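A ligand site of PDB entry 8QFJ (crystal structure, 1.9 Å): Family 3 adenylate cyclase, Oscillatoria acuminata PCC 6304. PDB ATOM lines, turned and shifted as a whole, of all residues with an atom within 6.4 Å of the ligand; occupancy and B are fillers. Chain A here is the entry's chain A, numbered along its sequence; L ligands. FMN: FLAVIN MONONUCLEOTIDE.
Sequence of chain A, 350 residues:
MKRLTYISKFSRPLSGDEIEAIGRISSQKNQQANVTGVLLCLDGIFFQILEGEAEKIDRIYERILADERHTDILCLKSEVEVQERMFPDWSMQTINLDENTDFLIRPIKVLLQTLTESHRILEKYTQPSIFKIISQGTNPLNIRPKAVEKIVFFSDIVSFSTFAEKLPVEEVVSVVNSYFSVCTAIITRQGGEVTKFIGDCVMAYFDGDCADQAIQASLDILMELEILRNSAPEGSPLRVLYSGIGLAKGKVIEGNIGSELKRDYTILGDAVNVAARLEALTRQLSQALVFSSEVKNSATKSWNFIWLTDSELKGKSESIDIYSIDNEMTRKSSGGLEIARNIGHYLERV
An oxygen (O1P) of the ligand is in salt-bridge range of the side-chain amino group (NZ) of Lys 29 (3.4 Å). The side-chain amide oxygen (OD1) of Asn 30 is in hydrogen-bond range of a nitrogen (N3) of the ligand. The guanidinium group (NH1) of Arg 63 lies within hydrogen-bond range of an oxygen (O2) of the ligand, at 2.6 Å. An oxygen (O2') of the ligand lies within hydrogen-bond range of the side-chain carboxylate (OD2) of Asp 67, at 3.4 Å. A nitrogen (N5) of the ligand sits at hydrogen-bond distance from the side-chain amide nitrogen (NE2) of Gln 48 (3.0 Å). An oxygen (O2') of the ligand sits at hydrogen-bond distance from the backbone carbonyl oxygen of Arg 63, at 3.2 Å.
Residues that only touch the ligand: Tyr 6 (3.2 Å), Ile 22 (3.5 Å), Ser 26 (3.2 Å), Leu 39 (3.8 Å), Phe 46 (3.5 Å), Leu 50 (3.4 Å), Ile 60 (3.7 Å), Ile 64 (3.6 Å), Arg 69 (3.9 Å), His 70 (3.7 Å) and Met 92 (3.5 Å). Hydrophobic or aromatic side chains within 4 Å of the ligand: Ile 22, Leu 39, Phe 46, Leu 50, Ile 60, Ile 64, His 70 and Met 92. Along chain A the residues within 4 Å of the ligand span positions 6 to 92.
The backbone carbonyl oxygen (O) of Ile 64 sits at hydrogen-bond distance from a ring nitrogen (NE2) of His 70, 2.8 Å away. The backbone NH (N) of Phe 46 is in hydrogen-bond range of the backbone carbonyl oxygen (O) of Ser 8. O of Ser 26 lies close to OD1 of Asn 30, 3.5 Å away. The side-chain carboxylate (OD2) of Asp 67 lies within salt-bridge range of the guanidinium group (NH2) of Arg 69, at 2.6 Å. The backbone carbonyl oxygen (O) of Ser 91 is in hydrogen-bond range of the side-chain amide nitrogen (ND2) of Asn 30, 2.9 Å away. The backbone carbonyl oxygen (O) of Ile 22 sits at hydrogen-bond distance from the side-chain hydroxyl (OG) of Ser 26 (2.6 Å). A ring nitrogen (ND1) of His 70 sits at hydrogen-bond distance from the side-chain hydroxyl of Ser 8 (2.8 Å). O of Asn 30 is in hydrogen-bond range of N of Val 35.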
ATOM      1  N   TYR A   6      -6.158 -21.864  22.803  1.00  0.00           N
ATOM      2  CA  TYR A   6      -5.496 -21.709  21.511  1.00  0.00           C
ATOM      3  C   TYR A   6      -6.468 -21.079  20.522  1.00  0.00           C
ATOM      4  O   TYR A   6      -7.692 -21.132  20.688  1.00  0.00           O
ATOM      5  CB  TYR A   6      -4.966 -23.061  20.983  1.00  0.00           C
ATOM      6  CG  TYR A   6      -5.994 -23.948  20.328  1.00  0.00           C
ATOM      7  CD1 TYR A   6      -6.425 -23.723  19.014  1.00  0.00           C
ATOM      8  CD2 TYR A   6      -6.538 -25.040  21.000  1.00  0.00           C
ATOM      9  CE1 TYR A   6      -7.364 -24.539  18.419  1.00  0.00           C
ATOM     10  CE2 TYR A   6      -7.478 -25.857  20.404  1.00  0.00           C
ATOM     11  CZ  TYR A   6      -7.886 -25.606  19.113  1.00  0.00           C
ATOM     12  OH  TYR A   6      -8.826 -26.413  18.521  1.00  0.00           O
ATOM     13  N   SER A   8      -6.838 -20.594  16.038  1.00  0.00           N
ATOM     14  CA  SER A   8      -6.361 -21.120  14.757  1.00  0.00           C
ATOM     15  C   SER A   8      -7.186 -20.512  13.639  1.00  0.00           C
ATOM     16  O   SER A   8      -8.193 -19.832  13.866  1.00  0.00           O
ATOM     17  CB  SER A   8      -6.438 -22.654  14.721  1.00  0.00           C
ATOM     18  OG  SER A   8      -7.774 -23.098  14.866  1.00  0.00           O
ATOM     19  N   LEU A  14     -15.718 -23.494   6.002  1.00  0.00           N
ATOM     20  CA  LEU A  14     -16.418 -24.527   6.750  1.00  0.00           C
ATOM     21  C   LEU A  14     -17.866 -24.106   6.936  1.00  0.00           C
ATOM     22  O   LEU A  14     -18.136 -23.041   7.490  1.00  0.00           O
ATOM     23  CB  LEU A  14     -15.755 -24.753   8.113  1.00  0.00           C
ATOM     24  CG  LEU A  14     -14.332 -25.311   8.111  1.00  0.00           C
ATOM     25  CD1 LEU A  14     -13.805 -25.429   9.538  1.00  0.00           C
ATOM     26  CD2 LEU A  14     -14.275 -26.660   7.415  1.00  0.00           C
ATOM     27  N   ILE A  22     -17.788 -31.053  13.931  1.00  0.00           N
ATOM     28  CA  ILE A  22     -16.648 -30.986  14.855  1.00  0.00           C
ATOM     29  C   ILE A  22     -17.143 -30.892  16.292  1.00  0.00           C
ATOM     30  O   ILE A  22     -16.590 -31.531  17.190  1.00  0.00           O
ATOM     31  CB  ILE A  22     -15.724 -29.800  14.488  1.00  0.00           C
ATOM     32  CG1 ILE A  22     -15.237 -29.923  13.044  1.00  0.00           C
ATOM     33  CG2 ILE A  22     -14.541 -29.742  15.450  1.00  0.00           C
ATOM     34  CD1 ILE A  22     -14.622 -28.658  12.503  1.00  0.00           C
ATOM     35  N   ILE A  25     -18.661 -34.637  17.513  1.00  0.00           N
ATOM     36  CA  ILE A  25     -17.646 -35.652  17.759  1.00  0.00           C
ATOM     37  C   ILE A  25     -16.716 -35.215  18.894  1.00  0.00           C
ATOM     38  O   ILE A  25     -16.319 -36.034  19.730  1.00  0.00           O
ATOM     39  CB  ILE A  25     -16.881 -35.974  16.462  1.00  0.00           C
ATOM     40  CG1 ILE A  25     -17.839 -36.586  15.434  1.00  0.00           C
ATOM     41  CG2 ILE A  25     -15.733 -36.944  16.724  1.00  0.00           C
ATOM     42  CD1 ILE A  25     -18.292 -35.652  14.335  1.00  0.00           C
ATOM     43  N   SER A  26     -16.375 -33.926  18.958  1.00  0.00           N
ATOM     44  CA  SER A  26     -15.600 -33.435  20.093  1.00  0.00           C
ATOM     45  C   SER A  26     -16.320 -33.717  21.407  1.00  0.00           C
ATOM     46  O   SER A  26     -15.704 -34.139  22.396  1.00  0.00           O
ATOM     47  CB  SER A  26     -15.335 -31.936  19.951  1.00  0.00           C
ATOM     48  OG  SER A  26     -14.563 -31.650  18.796  1.00  0.00           O
ATOM     49  N   SER A  27     -17.642 -33.500  21.436  1.00  0.00           N
ATOM     50  CA  SER A  27     -18.414 -33.744  22.658  1.00  0.00           C
ATOM     51  C   SER A  27     -18.333 -35.212  23.062  1.00  0.00           C
ATOM     52  O   SER A  27     -18.131 -35.526  24.246  1.00  0.00           O
ATOM     53  CB  SER A  27     -19.863 -33.326  22.438  1.00  0.00           C
ATOM     54  OG  SER A  27     -20.557 -33.233  23.675  1.00  0.00           O
ATOM     55  N   LYS A  29     -16.064 -37.473  22.415  1.00  0.00           N
ATOM     56  CA  LYS A  29     -14.728 -37.884  22.846  1.00  0.00           C
ATOM     57  C   LYS A  29     -14.308 -37.157  24.119  1.00  0.00           C
ATOM     58  O   LYS A  29     -13.638 -37.743  24.976  1.00  0.00           O
ATOM     59  CB  LYS A  29     -13.720 -37.646  21.724  1.00  0.00           C
ATOM     60  CG  LYS A  29     -14.143 -38.257  20.388  1.00  0.00           C
ATOM     61  CD  LYS A  29     -12.992 -38.373  19.407  1.00  0.00           C
ATOM     62  CE  LYS A  29     -12.090 -39.556  19.723  1.00  0.00           C
ATOM     63  NZ  LYS A  29     -10.937 -39.620  18.779  1.00  0.00           N
ATOM     64  N   ASN A  30     -14.686 -35.888  24.258  1.00  0.00           N
ATOM     65  CA  ASN A  30     -14.363 -35.154  25.487  1.00  0.00           C
ATOM     66  C   ASN A  30     -15.110 -35.727  26.687  1.00  0.00           C
ATOM     67  O   ASN A  30     -14.535 -35.865  27.766  1.00  0.00           O
ATOM     68  CB  ASN A  30     -14.698 -33.675  25.317  1.00  0.00           C
ATOM     69  CG  ASN A  30     -13.648 -32.924  24.537  1.00  0.00           C
ATOM     70  OD1 ASN A  30     -12.683 -33.510  24.046  1.00  0.00           O
ATOM     71  ND2 ASN A  30     -13.813 -31.615  24.436  1.00  0.00           N
ATOM     72  N   VAL A  35     -13.063 -34.450  29.789  1.00  0.00           N
ATOM     73  CA  VAL A  35     -12.690 -33.120  29.321  1.00  0.00           C
ATOM     74  C   VAL A  35     -13.944 -32.270  29.142  1.00  0.00           C
ATOM     75  O   VAL A  35     -14.955 -32.730  28.603  1.00  0.00           O
ATOM     76  CB  VAL A  35     -11.891 -33.203  28.011  1.00  0.00           C
ATOM     77  CG1 VAL A  35     -11.771 -31.830  27.361  1.00  0.00           C
ATOM     78  CG2 VAL A  35     -10.517 -33.818  28.269  1.00  0.00           C
ATOM     79  N   LEU A  39     -15.814 -24.287  22.257  1.00  0.00           N
ATOM     80  CA  LEU A  39     -15.230 -24.077  20.940  1.00  0.00           C
ATOM     81  C   LEU A  39     -15.972 -22.931  20.258  1.00  0.00           C
ATOM     82  O   LEU A  39     -17.142 -23.062  19.903  1.00  0.00           O
ATOM     83  CB  LEU A  39     -15.303 -25.358  20.108  1.00  0.00           C
ATOM     84  CG  LEU A  39     -15.010 -25.265  18.606  1.00  0.00           C
ATOM     85  CD1 LEU A  39     -13.540 -24.988  18.357  1.00  0.00           C
ATOM     86  CD2 LEU A  39     -15.442 -26.554  17.915  1.00  0.00           C
ATOM     87  N   PHE A  46     -10.969 -20.138  14.739  1.00  0.00           N
ATOM     88  CA  PHE A  46     -11.362 -20.986  15.854  1.00  0.00           C
ATOM     89  C   PHE A  46     -10.701 -20.457  17.134  1.00  0.00           C
ATOM     90  O   PHE A  46      -9.549 -20.026  17.118  1.00  0.00           O
ATOM     91  CB  PHE A  46     -10.952 -22.442  15.648  1.00  0.00           C
ATOM     92  CG  PHE A  46     -11.830 -23.196  14.682  1.00  0.00           C
ATOM     93  CD1 PHE A  46     -13.195 -23.328  14.900  1.00  0.00           C
ATOM     94  CD2 PHE A  46     -11.284 -23.824  13.566  1.00  0.00           C
ATOM     95  CE1 PHE A  46     -13.995 -24.032  14.024  1.00  0.00           C
ATOM     96  CE2 PHE A  46     -12.074 -24.527  12.687  1.00  0.00           C
ATOM     97  CZ  PHE A  46     -13.438 -24.633  12.923  1.00  0.00           C
ATOM     98  N   PHE A  47     -11.445 -20.488  18.227  1.00  0.00           N
ATOM     99  CA  PHE A  47     -10.930 -20.263  19.567  1.00  0.00           C
ATOM    100  C   PHE A  47     -11.345 -21.486  20.376  1.00  0.00           C
ATOM    101  O   PHE A  47     -12.514 -21.881  20.310  1.00  0.00           O
ATOM    102  CB  PHE A  47     -11.525 -19.011  20.226  1.00  0.00           C
ATOM    103  CG  PHE A  47     -11.209 -17.739  19.506  1.00  0.00           C
ATOM    104  CD1 PHE A  47     -10.188 -16.916  19.937  1.00  0.00           C
ATOM    105  CD2 PHE A  47     -11.954 -17.343  18.408  1.00  0.00           C
ATOM    106  CE1 PHE A  47      -9.883 -15.739  19.279  1.00  0.00           C
ATOM    107  CE2 PHE A  47     -11.669 -16.159  17.758  1.00  0.00           C
ATOM    108  CZ  PHE A  47     -10.635 -15.356  18.189  1.00  0.00           C
ATOM    109  N   GLN A  48     -10.428 -22.094  21.127  1.00  0.00           N
ATOM    110  CA  GLN A  48     -10.928 -23.172  22.018  1.00  0.00           C
ATOM    111  C   GLN A  48     -10.322 -23.106  23.412  1.00  0.00           C
ATOM    112  O   GLN A  48      -9.176 -22.695  23.523  1.00  0.00           O
ATOM    113  CB  GLN A  48     -10.680 -24.595  21.490  1.00  0.00           C
ATOM    114  CG  GLN A  48     -11.466 -25.600  22.328  1.00  0.00           C
ATOM    115  CD  GLN A  48     -11.414 -27.095  22.167  1.00  0.00           C
ATOM    116  OE1 GLN A  48     -11.955 -27.752  23.026  1.00  0.00           O
ATOM    117  NE2 GLN A  48     -10.817 -27.659  21.120  1.00  0.00           N
ATOM    118  N   LEU A  50      -9.868 -25.782  26.690  1.00  0.00           N
ATOM    119  CA  LEU A  50      -9.938 -27.227  26.930  1.00  0.00           C
ATOM    120  C   LEU A  50      -9.252 -27.542  28.247  1.00  0.00           C
ATOM    121  O   LEU A  50      -8.133 -27.089  28.478  1.00  0.00           O
ATOM    122  CB  LEU A  50      -9.284 -27.996  25.781  1.00  0.00           C
ATOM    123  CG  LEU A  50      -9.629 -29.467  25.596  1.00  0.00           C
ATOM    124  CD1 LEU A  50     -11.008 -29.654  25.048  1.00  0.00           C
ATOM    125  CD2 LEU A  50      -8.616 -30.103  24.660  1.00  0.00           C
ATOM    126  N   ILE A  60      -5.175 -35.032  23.447  1.00  0.00           N
ATOM    127  CA  ILE A  60      -6.231 -34.400  22.660  1.00  0.00           C
ATOM    128  C   ILE A  60      -5.674 -33.254  21.827  1.00  0.00           C
ATOM    129  O   ILE A  60      -5.964 -33.132  20.633  1.00  0.00           O
ATOM    130  CB  ILE A  60      -7.383 -33.932  23.564  1.00  0.00           C
ATOM    131  CG1 ILE A  60      -8.058 -35.146  24.227  1.00  0.00           C
ATOM    132  CG2 ILE A  60      -8.394 -33.127  22.773  1.00  0.00           C
ATOM    133  CD1 ILE A  60      -8.800 -34.814  25.498  1.00  0.00           C
ATOM    134  N   ARG A  63      -3.760 -34.500  18.546  1.00  0.00           N
ATOM    135  CA  ARG A  63      -4.546 -34.851  17.371  1.00  0.00           C
ATOM    136  C   ARG A  63      -5.374 -33.681  16.854  1.00  0.00           C
ATOM    137  O   ARG A  63      -5.762 -33.690  15.683  1.00  0.00           O
ATOM    138  CB  ARG A  63      -5.437 -36.060  17.688  1.00  0.00           C
ATOM    139  CG  ARG A  63      -6.906 -35.735  17.937  1.00  0.00           C
ATOM    140  CD  ARG A  63      -7.681 -37.004  18.264  1.00  0.00           C
ATOM    141  NE  ARG A  63      -7.587 -37.380  19.680  1.00  0.00           N
ATOM    142  CZ  ARG A  63      -8.519 -37.119  20.584  1.00  0.00           C
ATOM    143  NH1 ARG A  63      -9.585 -36.380  20.301  1.00  0.00           N
ATOM    144  NH2 ARG A  63      -8.373 -37.601  21.819  1.00  0.00           N
ATOM    145  N   ILE A  64      -5.643 -32.679  17.694  1.00  0.00           N
ATOM    146  CA  ILE A  64      -6.194 -31.425  17.205  1.00  0.00           C
ATOM    147  C   ILE A  64      -5.217 -30.752  16.260  1.00  0.00           C
ATOM    148  O   ILE A  64      -5.595 -30.219  15.209  1.00  0.00           O
ATOM    149  CB  ILE A  64      -6.581 -30.501  18.385  1.00  0.00           C
ATOM    150  CG1 ILE A  64      -7.745 -31.112  19.168  1.00  0.00           C
ATOM    151  CG2 ILE A  64      -6.917 -29.102  17.885  1.00  0.00           C
ATOM    152  CD1 ILE A  64      -7.965 -30.490  20.530  1.00  0.00           C
ATOM    153  N   LEU A  65      -3.933 -30.751  16.616  1.00  0.00           N
ATOM    154  CA  LEU A  65      -2.901 -30.226  15.717  1.00  0.00           C
ATOM    155  C   LEU A  65      -2.809 -31.031  14.435  1.00  0.00           C
ATOM    156  O   LEU A  65      -2.316 -30.517  13.426  1.00  0.00           O
ATOM    157  CB  LEU A  65      -1.543 -30.223  16.433  1.00  0.00           C
ATOM    158  CG  LEU A  65      -1.411 -29.332  17.661  1.00  0.00           C
ATOM    159  CD1 LEU A  65       0.063 -29.168  18.041  1.00  0.00           C
ATOM    160  CD2 LEU A  65      -2.046 -27.962  17.440  1.00  0.00           C
ATOM    161  N   ALA A  66      -3.273 -32.279  14.444  1.00  0.00           N
ATOM    162  CA  ALA A  66      -3.229 -33.144  13.268  1.00  0.00           C
ATOM    163  C   ALA A  66      -4.417 -32.963  12.349  1.00  0.00           C
ATOM    164  O   ALA A  66      -4.456 -33.582  11.274  1.00  0.00           O
ATOM    165  CB  ALA A  66      -3.140 -34.611  13.703  1.00  0.00           C
ATOM    166  N   ASP A  67      -5.394 -32.142  12.730  1.00  0.00           N
ATOM    167  CA  ASP A  67      -6.594 -31.966  11.922  1.00  0.00           C
ATOM    168  C   ASP A  67      -6.331 -30.984  10.791  1.00  0.00           C
ATOM    169  O   ASP A  67      -5.837 -29.874  11.014  1.00  0.00           O
ATOM    170  CB  ASP A  67      -7.758 -31.478  12.793  1.00  0.00           C
ATOM    171  CG  ASP A  67      -9.105 -31.582  12.097  1.00  0.00           C
ATOM    172  OD1 ASP A  67      -9.217 -31.123  10.942  1.00  0.00           O
ATOM    173  OD2 ASP A  67     -10.042 -32.131  12.708  1.00  0.00           O
ATOM    174  N   ARG A  69      -8.428 -29.342   8.935  1.00  0.00           N
ATOM    175  CA  ARG A  69      -9.410 -28.290   8.713  1.00  0.00           C
ATOM    176  C   ARG A  69      -9.048 -26.960   9.361  1.00  0.00           C
ATOM    177  O   ARG A  69      -9.782 -25.986   9.169  1.00  0.00           O
ATOM    178  CB  ARG A  69     -10.793 -28.734   9.200  1.00  0.00           C
ATOM    179  CG  ARG A  69     -11.491 -29.710   8.273  1.00  0.00           C
ATOM    180  CD  ARG A  69     -12.626 -30.450   8.974  1.00  0.00           C
ATOM    181  NE  ARG A  69     -12.146 -31.262  10.091  1.00  0.00           N
ATOM    182  CZ  ARG A  69     -12.946 -31.917  10.922  1.00  0.00           C
ATOM    183  NH1 ARG A  69     -14.255 -31.831  10.841  1.00  0.00           N
ATOM    184  NH2 ARG A  69     -12.394 -32.694  11.854  1.00  0.00           N
ATOM    185  N   HIS A  70      -7.953 -26.882  10.117  1.00  0.00           N
ATOM    186  CA  HIS A  70      -7.483 -25.586  10.601  1.00  0.00           C
ATOM    187  C   HIS A  70      -5.966 -25.544  10.592  1.00  0.00           C
ATOM    188  O   HIS A  70      -5.292 -26.581  10.642  1.00  0.00           O
ATOM    189  CB  HIS A  70      -8.036 -25.251  12.000  1.00  0.00           C
ATOM    190  CG  HIS A  70      -7.568 -26.170  13.088  1.00  0.00           C
ATOM    191  ND1 HIS A  70      -7.611 -25.809  14.414  1.00  0.00           N
ATOM    192  CD2 HIS A  70      -7.062 -27.420  13.047  1.00  0.00           C
ATOM    193  CE1 HIS A  70      -7.140 -26.801  15.151  1.00  0.00           C
ATOM    194  NE2 HIS A  70      -6.801 -27.790  14.347  1.00  0.00           N
ATOM    195  N   SER A  91     -19.000 -30.804  28.016  1.00  0.00           N
ATOM    196  CA  SER A  91     -17.972 -31.577  27.339  1.00  0.00           C
ATOM    197  C   SER A  91     -17.400 -30.841  26.123  1.00  0.00           C
ATOM    198  O   SER A  91     -16.219 -30.928  25.829  1.00  0.00           O
ATOM    199  CB  SER A  91     -18.530 -32.922  26.888  1.00  0.00           C
ATOM    200  OG  SER A  91     -19.229 -33.563  27.954  1.00  0.00           O
ATOM    201  N   MET A  92     -18.293 -30.153  25.390  1.00  0.00           N
ATOM    202  CA  MET A  92     -17.895 -29.266  24.318  1.00  0.00           C
ATOM    203  C   MET A  92     -19.123 -28.426  23.954  1.00  0.00           C
ATOM    204  O   MET A  92     -20.064 -28.959  23.360  1.00  0.00           O
ATOM    205  CB  MET A  92     -17.376 -30.048  23.086  1.00  0.00           C
ATOM    206  CG  MET A  92     -17.088 -29.161  21.831  1.00  0.00           C
ATOM    207  SD  MET A  92     -15.581 -28.135  21.846  1.00  0.00           S
ATOM    208  CE  MET A  92     -14.559 -28.910  23.058  1.00  0.00           C
HETATM  209  N1  FMN L   1     -11.556 -33.706  19.053  1.00  0.00           N
HETATM  210  C2  FMN L   1     -11.728 -34.039  20.476  1.00  0.00           C
HETATM  211  O2  FMN L   1     -11.797 -35.172  20.824  1.00  0.00           O
HETATM  212  N3  FMN L   1     -11.810 -32.952  21.482  1.00  0.00           N
HETATM  213  C4  FMN L   1     -11.715 -31.563  21.064  1.00  0.00           C
HETATM  214  O4  FMN L   1     -11.778 -30.689  21.856  1.00  0.00           O
HETATM  215  C4A FMN L   1     -11.534 -31.243  19.589  1.00  0.00           C
HETATM  216  N5  FMN L   1     -11.450 -29.871  19.158  1.00  0.00           N
HETATM  217  C5A FMN L   1     -11.270 -29.552  17.717  1.00  0.00           C
HETATM  218  C6  FMN L   1     -11.184 -28.202  17.322  1.00  0.00           C
HETATM  219  C7  FMN L   1     -11.023 -27.864  15.979  1.00  0.00           C
HETATM  220  C7M FMN L   1     -10.972 -26.340  15.911  1.00  0.00           C
HETATM  221  C8  FMN L   1     -10.950 -28.892  15.017  1.00  0.00           C
HETATM  222  C8M FMN L   1     -10.770 -28.445  13.571  1.00  0.00           C
HETATM  223  C9  FMN L   1     -11.040 -30.220  15.409  1.00  0.00           C
HETATM  224  C9A FMN L   1     -11.197 -30.570  16.757  1.00  0.00           C
HETATM  225  N10 FMN L   1     -11.288 -32.011  17.202  1.00  0.00           N
HETATM  226  C10 FMN L   1     -11.458 -32.309  18.614  1.00  0.00           C
HETATM  227  C1' FMN L   1     -11.228 -33.111  16.265  1.00  0.00           C
HETATM  228  C2' FMN L   1      -9.944 -33.928  16.379  1.00  0.00           C
HETATM  229  O2' FMN L   1      -8.896 -33.239  15.755  1.00  0.00           O
HETATM  230  C3' FMN L   1     -10.132 -35.279  15.703  1.00  0.00           C
HETATM  231  O3' FMN L   1     -10.704 -35.078  14.436  1.00  0.00           O
HETATM  232  C4' FMN L   1     -11.059 -36.203  16.490  1.00  0.00           C
HETATM  233  O4' FMN L   1     -10.772 -36.140  17.861  1.00  0.00           O
HETATM  234  C5' FMN L   1     -10.863 -37.641  15.995  1.00  0.00           C
HETATM  235  O5' FMN L   1     -11.896 -38.460  16.476  1.00  0.00           O
HETATM  236  P   FMN L   1     -12.249 -39.842  15.634  1.00  0.00           P
HETATM  237  O1P FMN L   1     -13.139 -40.725  16.466  1.00  0.00           O
HETATM  238  O2P FMN L   1     -12.954 -39.476  14.350  1.00  0.00           O
HETATM  239  O3P FMN L   1     -10.965 -40.569  15.318  1.00  0.00           O
